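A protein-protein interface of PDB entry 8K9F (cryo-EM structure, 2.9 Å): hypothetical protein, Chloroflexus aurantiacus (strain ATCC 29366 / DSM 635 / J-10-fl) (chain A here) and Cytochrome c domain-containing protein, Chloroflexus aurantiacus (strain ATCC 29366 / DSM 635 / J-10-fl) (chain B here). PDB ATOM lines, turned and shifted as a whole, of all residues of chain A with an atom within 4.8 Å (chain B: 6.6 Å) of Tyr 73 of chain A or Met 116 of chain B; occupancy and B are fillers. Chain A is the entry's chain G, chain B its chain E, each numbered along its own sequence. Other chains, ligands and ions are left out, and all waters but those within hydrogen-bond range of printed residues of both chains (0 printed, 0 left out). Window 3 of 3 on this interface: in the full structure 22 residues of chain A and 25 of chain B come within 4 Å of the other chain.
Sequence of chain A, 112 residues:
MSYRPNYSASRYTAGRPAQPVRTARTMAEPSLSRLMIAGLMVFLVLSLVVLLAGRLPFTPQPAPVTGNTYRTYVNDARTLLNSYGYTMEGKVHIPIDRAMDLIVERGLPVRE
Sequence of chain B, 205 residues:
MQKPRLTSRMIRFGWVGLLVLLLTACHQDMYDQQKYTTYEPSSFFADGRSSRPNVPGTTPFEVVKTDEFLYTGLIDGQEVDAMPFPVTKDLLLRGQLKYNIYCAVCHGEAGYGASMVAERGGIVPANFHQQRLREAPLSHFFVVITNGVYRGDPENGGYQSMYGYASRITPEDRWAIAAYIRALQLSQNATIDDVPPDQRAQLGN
Of the 10 printed residues of chain A, 5 touch a printed residue of chain B.
Printed residues of chain A that touch a printed residue of chain B: Asn 68, Thr 69, Tyr 70, Tyr 73 and Ala 77.
Of the 13 printed residues of chain B, 5 touch a printed residue of chain A.
Hydrophobic or aromatic side chains of chain B that line the printed part of chain A: Ala 110 and Met 116.
Among the printed residues, 8 pairs touch across the chains.
Among the printed residues, no Asp or Glu carboxylate lies within 4 Å of a Lys or Arg side-chain nitrogen of the other chain.
Of the printed residues of chain B, Asn 68 of chain A touches Met 116 and Glu 119.
Of the printed residues of chain B, Thr 69 of chain A touches Met 116.
Of chain B, only Ser 115 and Met 116 come within 4 Å of Tyr 73 of chain A.
Of the printed residues of chain A, Glu 109 of chain B touches Ala 77.
Of the printed residues of chain A, Ala 110 of chain B touches Ala 77.
Of the printed residues of chain A, Ser 115 of chain B touches Tyr 73.
Printed residues of chain A within 4 Å of Met 116 of chain B: Asn 68 (3.3 Å), Thr 69 (3.7 Å), Tyr 70 (3.9 Å) and Tyr 73 (3.6 Å).
Arg 120 of chain B touches none of the printed residues of chain A.
The nearest residue of chain B that does not touch Tyr 73 of chain A is Glu 119 of chain B (4.2 Å).
The nearest printed residue of chain A that does not touch Met 116 of chain B is Arg 71 of chain A (6.2 Å).
NH1 of Arg 71 of chain A lies within hydrogen-bond range of OG1 of Thr 69 of chain A, at 3.3 Å.
The side-chain hydroxyl (OG) of Ser 115 of chain B lies close to the backbone NH (N) of Cys 106 of chain B (3.2 Å).
The side-chain hydroxyl (OG) of Ser 115 of chain B is in hydrogen-bond range of the backbone NH (N) of Val 117 of chain B (3.3 Å).
Among the printed residues, merely in contact across the chains: Asn 68 of chain A with Met 116 of chain B, Asn 68 of chain A with Glu 119 of chain B, Thr 69 of chain A with Met 116 of chain B, Tyr 70 of chain A with Met 116 of chain B, Tyr 73 of chain A with Ser 115 of chain B, Tyr 73 of chain A with Met 116 of chain B, Ala 77 of chain A with Glu 109 of chain B and Ala 77 of chain A with Ala 110 of chain B.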
ATOM      1  N   ASN A  68     -12.953  18.244  -3.782  1.00  0.00           N
ATOM      2  CA  ASN A  68     -14.149  18.762  -3.139  1.00  0.00           C
ATOM      3  C   ASN A  68     -14.663  19.984  -3.887  1.00  0.00           C
ATOM      4  O   ASN A  68     -13.905  20.689  -4.556  1.00  0.00           O
ATOM      5  CB  ASN A  68     -13.892  19.025  -1.637  1.00  0.00           C
ATOM      6  CG  ASN A  68     -13.737  17.754  -0.774  1.00  0.00           C
ATOM      7  OD1 ASN A  68     -14.202  16.660  -1.108  1.00  0.00           O
ATOM      8  ND2 ASN A  68     -13.049  17.915   0.351  1.00  0.00           N
ATOM      9  N   THR A  69     -15.964  20.192  -3.828  1.00  0.00           N
ATOM     10  CA  THR A  69     -16.596  21.346  -4.434  1.00  0.00           C
ATOM     11  C   THR A  69     -17.306  22.149  -3.351  1.00  0.00           C
ATOM     12  O   THR A  69     -17.328  21.771  -2.178  1.00  0.00           O
ATOM     13  CB  THR A  69     -17.543  20.911  -5.553  1.00  0.00           C
ATOM     14  OG1 THR A  69     -17.977  22.056  -6.294  1.00  0.00           O
ATOM     15  CG2 THR A  69     -18.736  20.184  -4.991  1.00  0.00           C
ATOM     16  N   TYR A  70     -17.871  23.285  -3.754  1.00  0.00           N
ATOM     17  CA  TYR A  70     -18.632  24.117  -2.832  1.00  0.00           C
ATOM     18  C   TYR A  70     -19.934  23.477  -2.389  1.00  0.00           C
ATOM     19  O   TYR A  70     -20.488  23.900  -1.372  1.00  0.00           O
ATOM     20  CB  TYR A  70     -18.946  25.474  -3.463  1.00  0.00           C
ATOM     21  CG  TYR A  70     -20.122  25.460  -4.419  1.00  0.00           C
ATOM     22  CD1 TYR A  70     -20.082  24.718  -5.592  1.00  0.00           C
ATOM     23  CD2 TYR A  70     -21.272  26.185  -4.143  1.00  0.00           C
ATOM     24  CE1 TYR A  70     -21.141  24.705  -6.465  1.00  0.00           C
ATOM     25  CE2 TYR A  70     -22.347  26.169  -5.008  1.00  0.00           C
ATOM     26  CZ  TYR A  70     -22.274  25.424  -6.169  1.00  0.00           C
ATOM     27  OH  TYR A  70     -23.334  25.404  -7.040  1.00  0.00           O
ATOM     28  N   ARG A  71     -20.431  22.479  -3.130  1.00  0.00           N
ATOM     29  CA  ARG A  71     -21.763  21.937  -2.883  1.00  0.00           C
ATOM     30  C   ARG A  71     -21.866  21.218  -1.551  1.00  0.00           C
ATOM     31  O   ARG A  71     -22.932  21.254  -0.938  1.00  0.00           O
ATOM     32  CB  ARG A  71     -22.178  20.989  -4.003  1.00  0.00           C
ATOM     33  CG  ARG A  71     -22.584  21.682  -5.271  1.00  0.00           C
ATOM     34  CD  ARG A  71     -22.716  20.712  -6.415  1.00  0.00           C
ATOM     35  NE  ARG A  71     -22.932  21.410  -7.675  1.00  0.00           N
ATOM     36  CZ  ARG A  71     -21.961  21.869  -8.449  1.00  0.00           C
ATOM     37  NH1 ARG A  71     -20.689  21.729  -8.116  1.00  0.00           N
ATOM     38  NH2 ARG A  71     -22.273  22.488  -9.584  1.00  0.00           N
ATOM     39  N   THR A  72     -20.787  20.576  -1.090  1.00  0.00           N
ATOM     40  CA  THR A  72     -20.835  19.834   0.170  1.00  0.00           C
ATOM     41  C   THR A  72     -21.074  20.770   1.351  1.00  0.00           C
ATOM     42  O   THR A  72     -22.006  20.566   2.143  1.00  0.00           O
ATOM     43  CB  THR A  72     -19.539  19.039   0.352  1.00  0.00           C
ATOM     44  OG1 THR A  72     -19.582  17.867  -0.471  1.00  0.00           O
ATOM     45  CG2 THR A  72     -19.352  18.606   1.806  1.00  0.00           C
ATOM     46  N   TYR A  73     -20.275  21.841   1.443  1.00  0.00           N
ATOM     47  CA  TYR A  73     -20.477  22.861   2.468  1.00  0.00           C
ATOM     48  C   TYR A  73     -21.810  23.569   2.301  1.00  0.00           C
ATOM     49  O   TYR A  73     -22.457  23.903   3.299  1.00  0.00           O
ATOM     50  CB  TYR A  73     -19.350  23.893   2.428  1.00  0.00           C
ATOM     51  CG  TYR A  73     -17.975  23.350   2.726  1.00  0.00           C
ATOM     52  CD1 TYR A  73     -17.745  22.560   3.848  1.00  0.00           C
ATOM     53  CD2 TYR A  73     -16.904  23.635   1.894  1.00  0.00           C
ATOM     54  CE1 TYR A  73     -16.485  22.067   4.127  1.00  0.00           C
ATOM     55  CE2 TYR A  73     -15.641  23.148   2.167  1.00  0.00           C
ATOM     56  CZ  TYR A  73     -15.439  22.364   3.281  1.00  0.00           C
ATOM     57  OH  TYR A  73     -14.178  21.880   3.545  1.00  0.00           O
ATOM     58  N   VAL A  74     -22.239  23.786   1.054  1.00  0.00           N
ATOM     59  CA  VAL A  74     -23.461  24.543   0.795  1.00  0.00           C
ATOM     60  C   VAL A  74     -24.683  23.761   1.261  1.00  0.00           C
ATOM     61  O   VAL A  74     -25.527  24.299   1.981  1.00  0.00           O
ATOM     62  CB  VAL A  74     -23.556  24.940  -0.691  1.00  0.00           C
ATOM     63  CG1 VAL A  74     -24.999  25.074  -1.164  1.00  0.00           C
ATOM     64  CG2 VAL A  74     -22.844  26.258  -0.907  1.00  0.00           C
ATOM     65  N   ASN A  75     -24.776  22.471   0.916  1.00  0.00           N
ATOM     66  CA  ASN A  75     -25.951  21.738   1.369  1.00  0.00           C
ATOM     67  C   ASN A  75     -25.841  21.329   2.832  1.00  0.00           C
ATOM     68  O   ASN A  75     -26.879  21.135   3.475  1.00  0.00           O
ATOM     69  CB  ASN A  75     -26.256  20.520   0.476  1.00  0.00           C
ATOM     70  CG  ASN A  75     -25.080  19.575   0.297  1.00  0.00           C
ATOM     71  OD1 ASN A  75     -24.395  19.197   1.244  1.00  0.00           O
ATOM     72  ND2 ASN A  75     -24.839  19.195  -0.949  1.00  0.00           N
ATOM     73  N   ASP A  76     -24.623  21.238   3.384  1.00  0.00           N
ATOM     74  CA  ASP A  76     -24.487  21.062   4.827  1.00  0.00           C
ATOM     75  C   ASP A  76     -25.026  22.271   5.583  1.00  0.00           C
ATOM     76  O   ASP A  76     -25.786  22.121   6.547  1.00  0.00           O
ATOM     77  CB  ASP A  76     -23.024  20.810   5.189  1.00  0.00           C
ATOM     78  CG  ASP A  76     -22.747  19.356   5.520  1.00  0.00           C
ATOM     79  OD1 ASP A  76     -23.711  18.566   5.591  1.00  0.00           O
ATOM     80  OD2 ASP A  76     -21.564  19.004   5.706  1.00  0.00           O
ATOM     81  N   ALA A  77     -24.689  23.480   5.131  1.00  0.00           N
ATOM     82  CA  ALA A  77     -25.231  24.680   5.760  1.00  0.00           C
ATOM     83  C   ALA A  77     -26.705  24.887   5.438  1.00  0.00           C
ATOM     84  O   ALA A  77     -27.419  25.505   6.229  1.00  0.00           O
ATOM     85  CB  ALA A  77     -24.427  25.906   5.337  1.00  0.00           C
ATOM     86  N   CYS B 106     -17.035  32.502   1.194  1.00  0.00           N
ATOM     87  CA  CYS B 106     -16.099  32.669   2.323  1.00  0.00           C
ATOM     88  C   CYS B 106     -16.743  33.210   3.606  1.00  0.00           C
ATOM     89  O   CYS B 106     -16.098  33.908   4.383  1.00  0.00           O
ATOM     90  CB  CYS B 106     -14.952  33.593   1.908  1.00  0.00           C
ATOM     91  SG  CYS B 106     -15.481  35.200   1.274  1.00  0.00           S
ATOM     92  N   GLY B 108     -20.027  31.064   4.456  1.00  0.00           N
ATOM     93  CA  GLY B 108     -20.979  29.982   4.654  1.00  0.00           C
ATOM     94  C   GLY B 108     -22.411  30.472   4.696  1.00  0.00           C
ATOM     95  O   GLY B 108     -22.710  31.578   5.143  1.00  0.00           O
ATOM     96  N   GLU B 109     -23.318  29.622   4.201  1.00  0.00           N
ATOM     97  CA  GLU B 109     -24.743  29.932   4.265  1.00  0.00           C
ATOM     98  C   GLU B 109     -25.239  29.951   5.705  1.00  0.00           C
ATOM     99  O   GLU B 109     -26.131  30.731   6.054  1.00  0.00           O
ATOM    100  CB  GLU B 109     -25.547  28.922   3.445  1.00  0.00           C
ATOM    101  CG  GLU B 109     -25.049  28.691   2.027  1.00  0.00           C
ATOM    102  CD  GLU B 109     -25.874  29.444   0.998  1.00  0.00           C
ATOM    103  OE1 GLU B 109     -26.782  28.831   0.403  1.00  0.00           O
ATOM    104  OE2 GLU B 109     -25.624  30.648   0.790  1.00  0.00           O
ATOM    105  N   ALA B 110     -24.671  29.096   6.558  1.00  0.00           N
ATOM    106  CA  ALA B 110     -25.003  29.147   7.975  1.00  0.00           C
ATOM    107  C   ALA B 110     -24.362  30.345   8.656  1.00  0.00           C
ATOM    108  O   ALA B 110     -24.849  30.794   9.697  1.00  0.00           O
ATOM    109  CB  ALA B 110     -24.578  27.855   8.664  1.00  0.00           C
ATOM    110  N   GLY B 113     -18.384  30.750   8.649  1.00  0.00           N
ATOM    111  CA  GLY B 113     -17.074  30.989   8.077  1.00  0.00           C
ATOM    112  C   GLY B 113     -16.566  29.858   7.208  1.00  0.00           C
ATOM    113  O   GLY B 113     -15.947  30.097   6.168  1.00  0.00           O
ATOM    114  N   ALA B 114     -16.840  28.623   7.618  1.00  0.00           N
ATOM    115  CA  ALA B 114     -16.321  27.428   6.960  1.00  0.00           C
ATOM    116  C   ALA B 114     -17.042  27.226   5.636  1.00  0.00           C
ATOM    117  O   ALA B 114     -18.097  26.593   5.572  1.00  0.00           O
ATOM    118  CB  ALA B 114     -16.489  26.216   7.866  1.00  0.00           C
ATOM    119  N   SER B 115     -16.456  27.760   4.573  1.00  0.00           N
ATOM    120  CA  SER B 115     -16.956  27.564   3.222  1.00  0.00           C
ATOM    121  C   SER B 115     -15.810  26.991   2.412  1.00  0.00           C
ATOM    122  O   SER B 115     -14.799  26.568   2.980  1.00  0.00           O
ATOM    123  CB  SER B 115     -17.425  28.862   2.592  1.00  0.00           C
ATOM    124  OG  SER B 115     -16.308  29.496   2.012  1.00  0.00           O
ATOM    125  N   MET B 116     -15.942  26.965   1.093  1.00  0.00           N
ATOM    126  CA  MET B 116     -14.905  26.313   0.320  1.00  0.00           C
ATOM    127  C   MET B 116     -13.835  27.291  -0.160  1.00  0.00           C
ATOM    128  O   MET B 116     -12.694  26.877  -0.385  1.00  0.00           O
ATOM    129  CB  MET B 116     -15.537  25.555  -0.849  1.00  0.00           C
ATOM    130  CG  MET B 116     -14.811  24.263  -1.115  1.00  0.00           C
ATOM    131  SD  MET B 116     -13.366  24.403  -2.128  1.00  0.00           S
ATOM    132  CE  MET B 116     -13.994  23.812  -3.624  1.00  0.00           C
ATOM    133  N   VAL B 117     -14.152  28.588  -0.261  1.00  0.00           N
ATOM    134  CA  VAL B 117     -13.111  29.595  -0.471  1.00  0.00           C
ATOM    135  C   VAL B 117     -12.171  29.647   0.722  1.00  0.00           C
ATOM    136  O   VAL B 117     -10.978  29.931   0.573  1.00  0.00           O
ATOM    137  CB  VAL B 117     -13.729  30.978  -0.735  1.00  0.00           C
ATOM    138  CG1 VAL B 117     -12.736  31.883  -1.451  1.00  0.00           C
ATOM    139  CG2 VAL B 117     -14.990  30.836  -1.544  1.00  0.00           C
ATOM    140  N   ALA B 118     -12.679  29.348   1.910  1.00  0.00           N
ATOM    141  CA  ALA B 118     -11.887  29.269   3.123  1.00  0.00           C
ATOM    142  C   ALA B 118     -11.034  28.009   3.202  1.00  0.00           C
ATOM    143  O   ALA B 118     -10.211  27.895   4.116  1.00  0.00           O
ATOM    144  CB  ALA B 118     -12.803  29.352   4.342  1.00  0.00           C
ATOM    145  N   GLU B 119     -11.211  27.054   2.287  1.00  0.00           N
ATOM    146  CA  GLU B 119     -10.412  25.838   2.324  1.00  0.00           C
ATOM    147  C   GLU B 119      -9.200  25.921   1.404  1.00  0.00           C
ATOM    148  O   GLU B 119      -8.101  25.520   1.803  1.00  0.00           O
ATOM    149  CB  GLU B 119     -11.262  24.620   1.931  1.00  0.00           C
ATOM    150  CG  GLU B 119     -10.481  23.308   1.781  1.00  0.00           C
ATOM    151  CD  GLU B 119     -10.961  22.444   0.641  1.00  0.00           C
ATOM    152  OE1 GLU B 119     -11.052  21.207   0.799  1.00  0.00           O
ATOM    153  OE2 GLU B 119     -11.151  22.994  -0.450  1.00  0.00           O
ATOM    154  N   ARG B 120      -9.364  26.460   0.197  1.00  0.00           N
ATOM    155  CA  ARG B 120      -8.261  26.666  -0.738  1.00  0.00           C
ATOM    156  C   ARG B 120      -7.783  28.108  -0.603  1.00  0.00           C
ATOM    157  O   ARG B 120      -8.471  29.043  -1.020  1.00  0.00           O
ATOM    158  CB  ARG B 120      -8.679  26.363  -2.174  1.00  0.00           C
ATOM    159  CG  ARG B 120      -9.912  25.501  -2.322  1.00  0.00           C
ATOM    160  CD  ARG B 120     -10.256  25.311  -3.794  1.00  0.00           C
ATOM    161  NE  ARG B 120      -9.111  24.876  -4.582  1.00  0.00           N
ATOM    162  CZ  ARG B 120      -8.922  23.637  -5.016  1.00  0.00           C
ATOM    163  NH1 ARG B 120      -9.809  22.683  -4.789  1.00  0.00           N
ATOM    164  NH2 ARG B 120      -7.819  23.351  -5.700  1.00  0.00           N
ATOM    165  N   GLY B 121      -6.607  28.286  -0.018  1.00  0.00           N
ATOM    166  CA  GLY B 121      -6.032  29.610   0.094  1.00  0.00           C
ATOM    167  C   GLY B 121      -5.735  30.052   1.510  1.00  0.00           C
ATOM    168  O   GLY B 121      -4.719  30.707   1.756  1.00  0.00           O
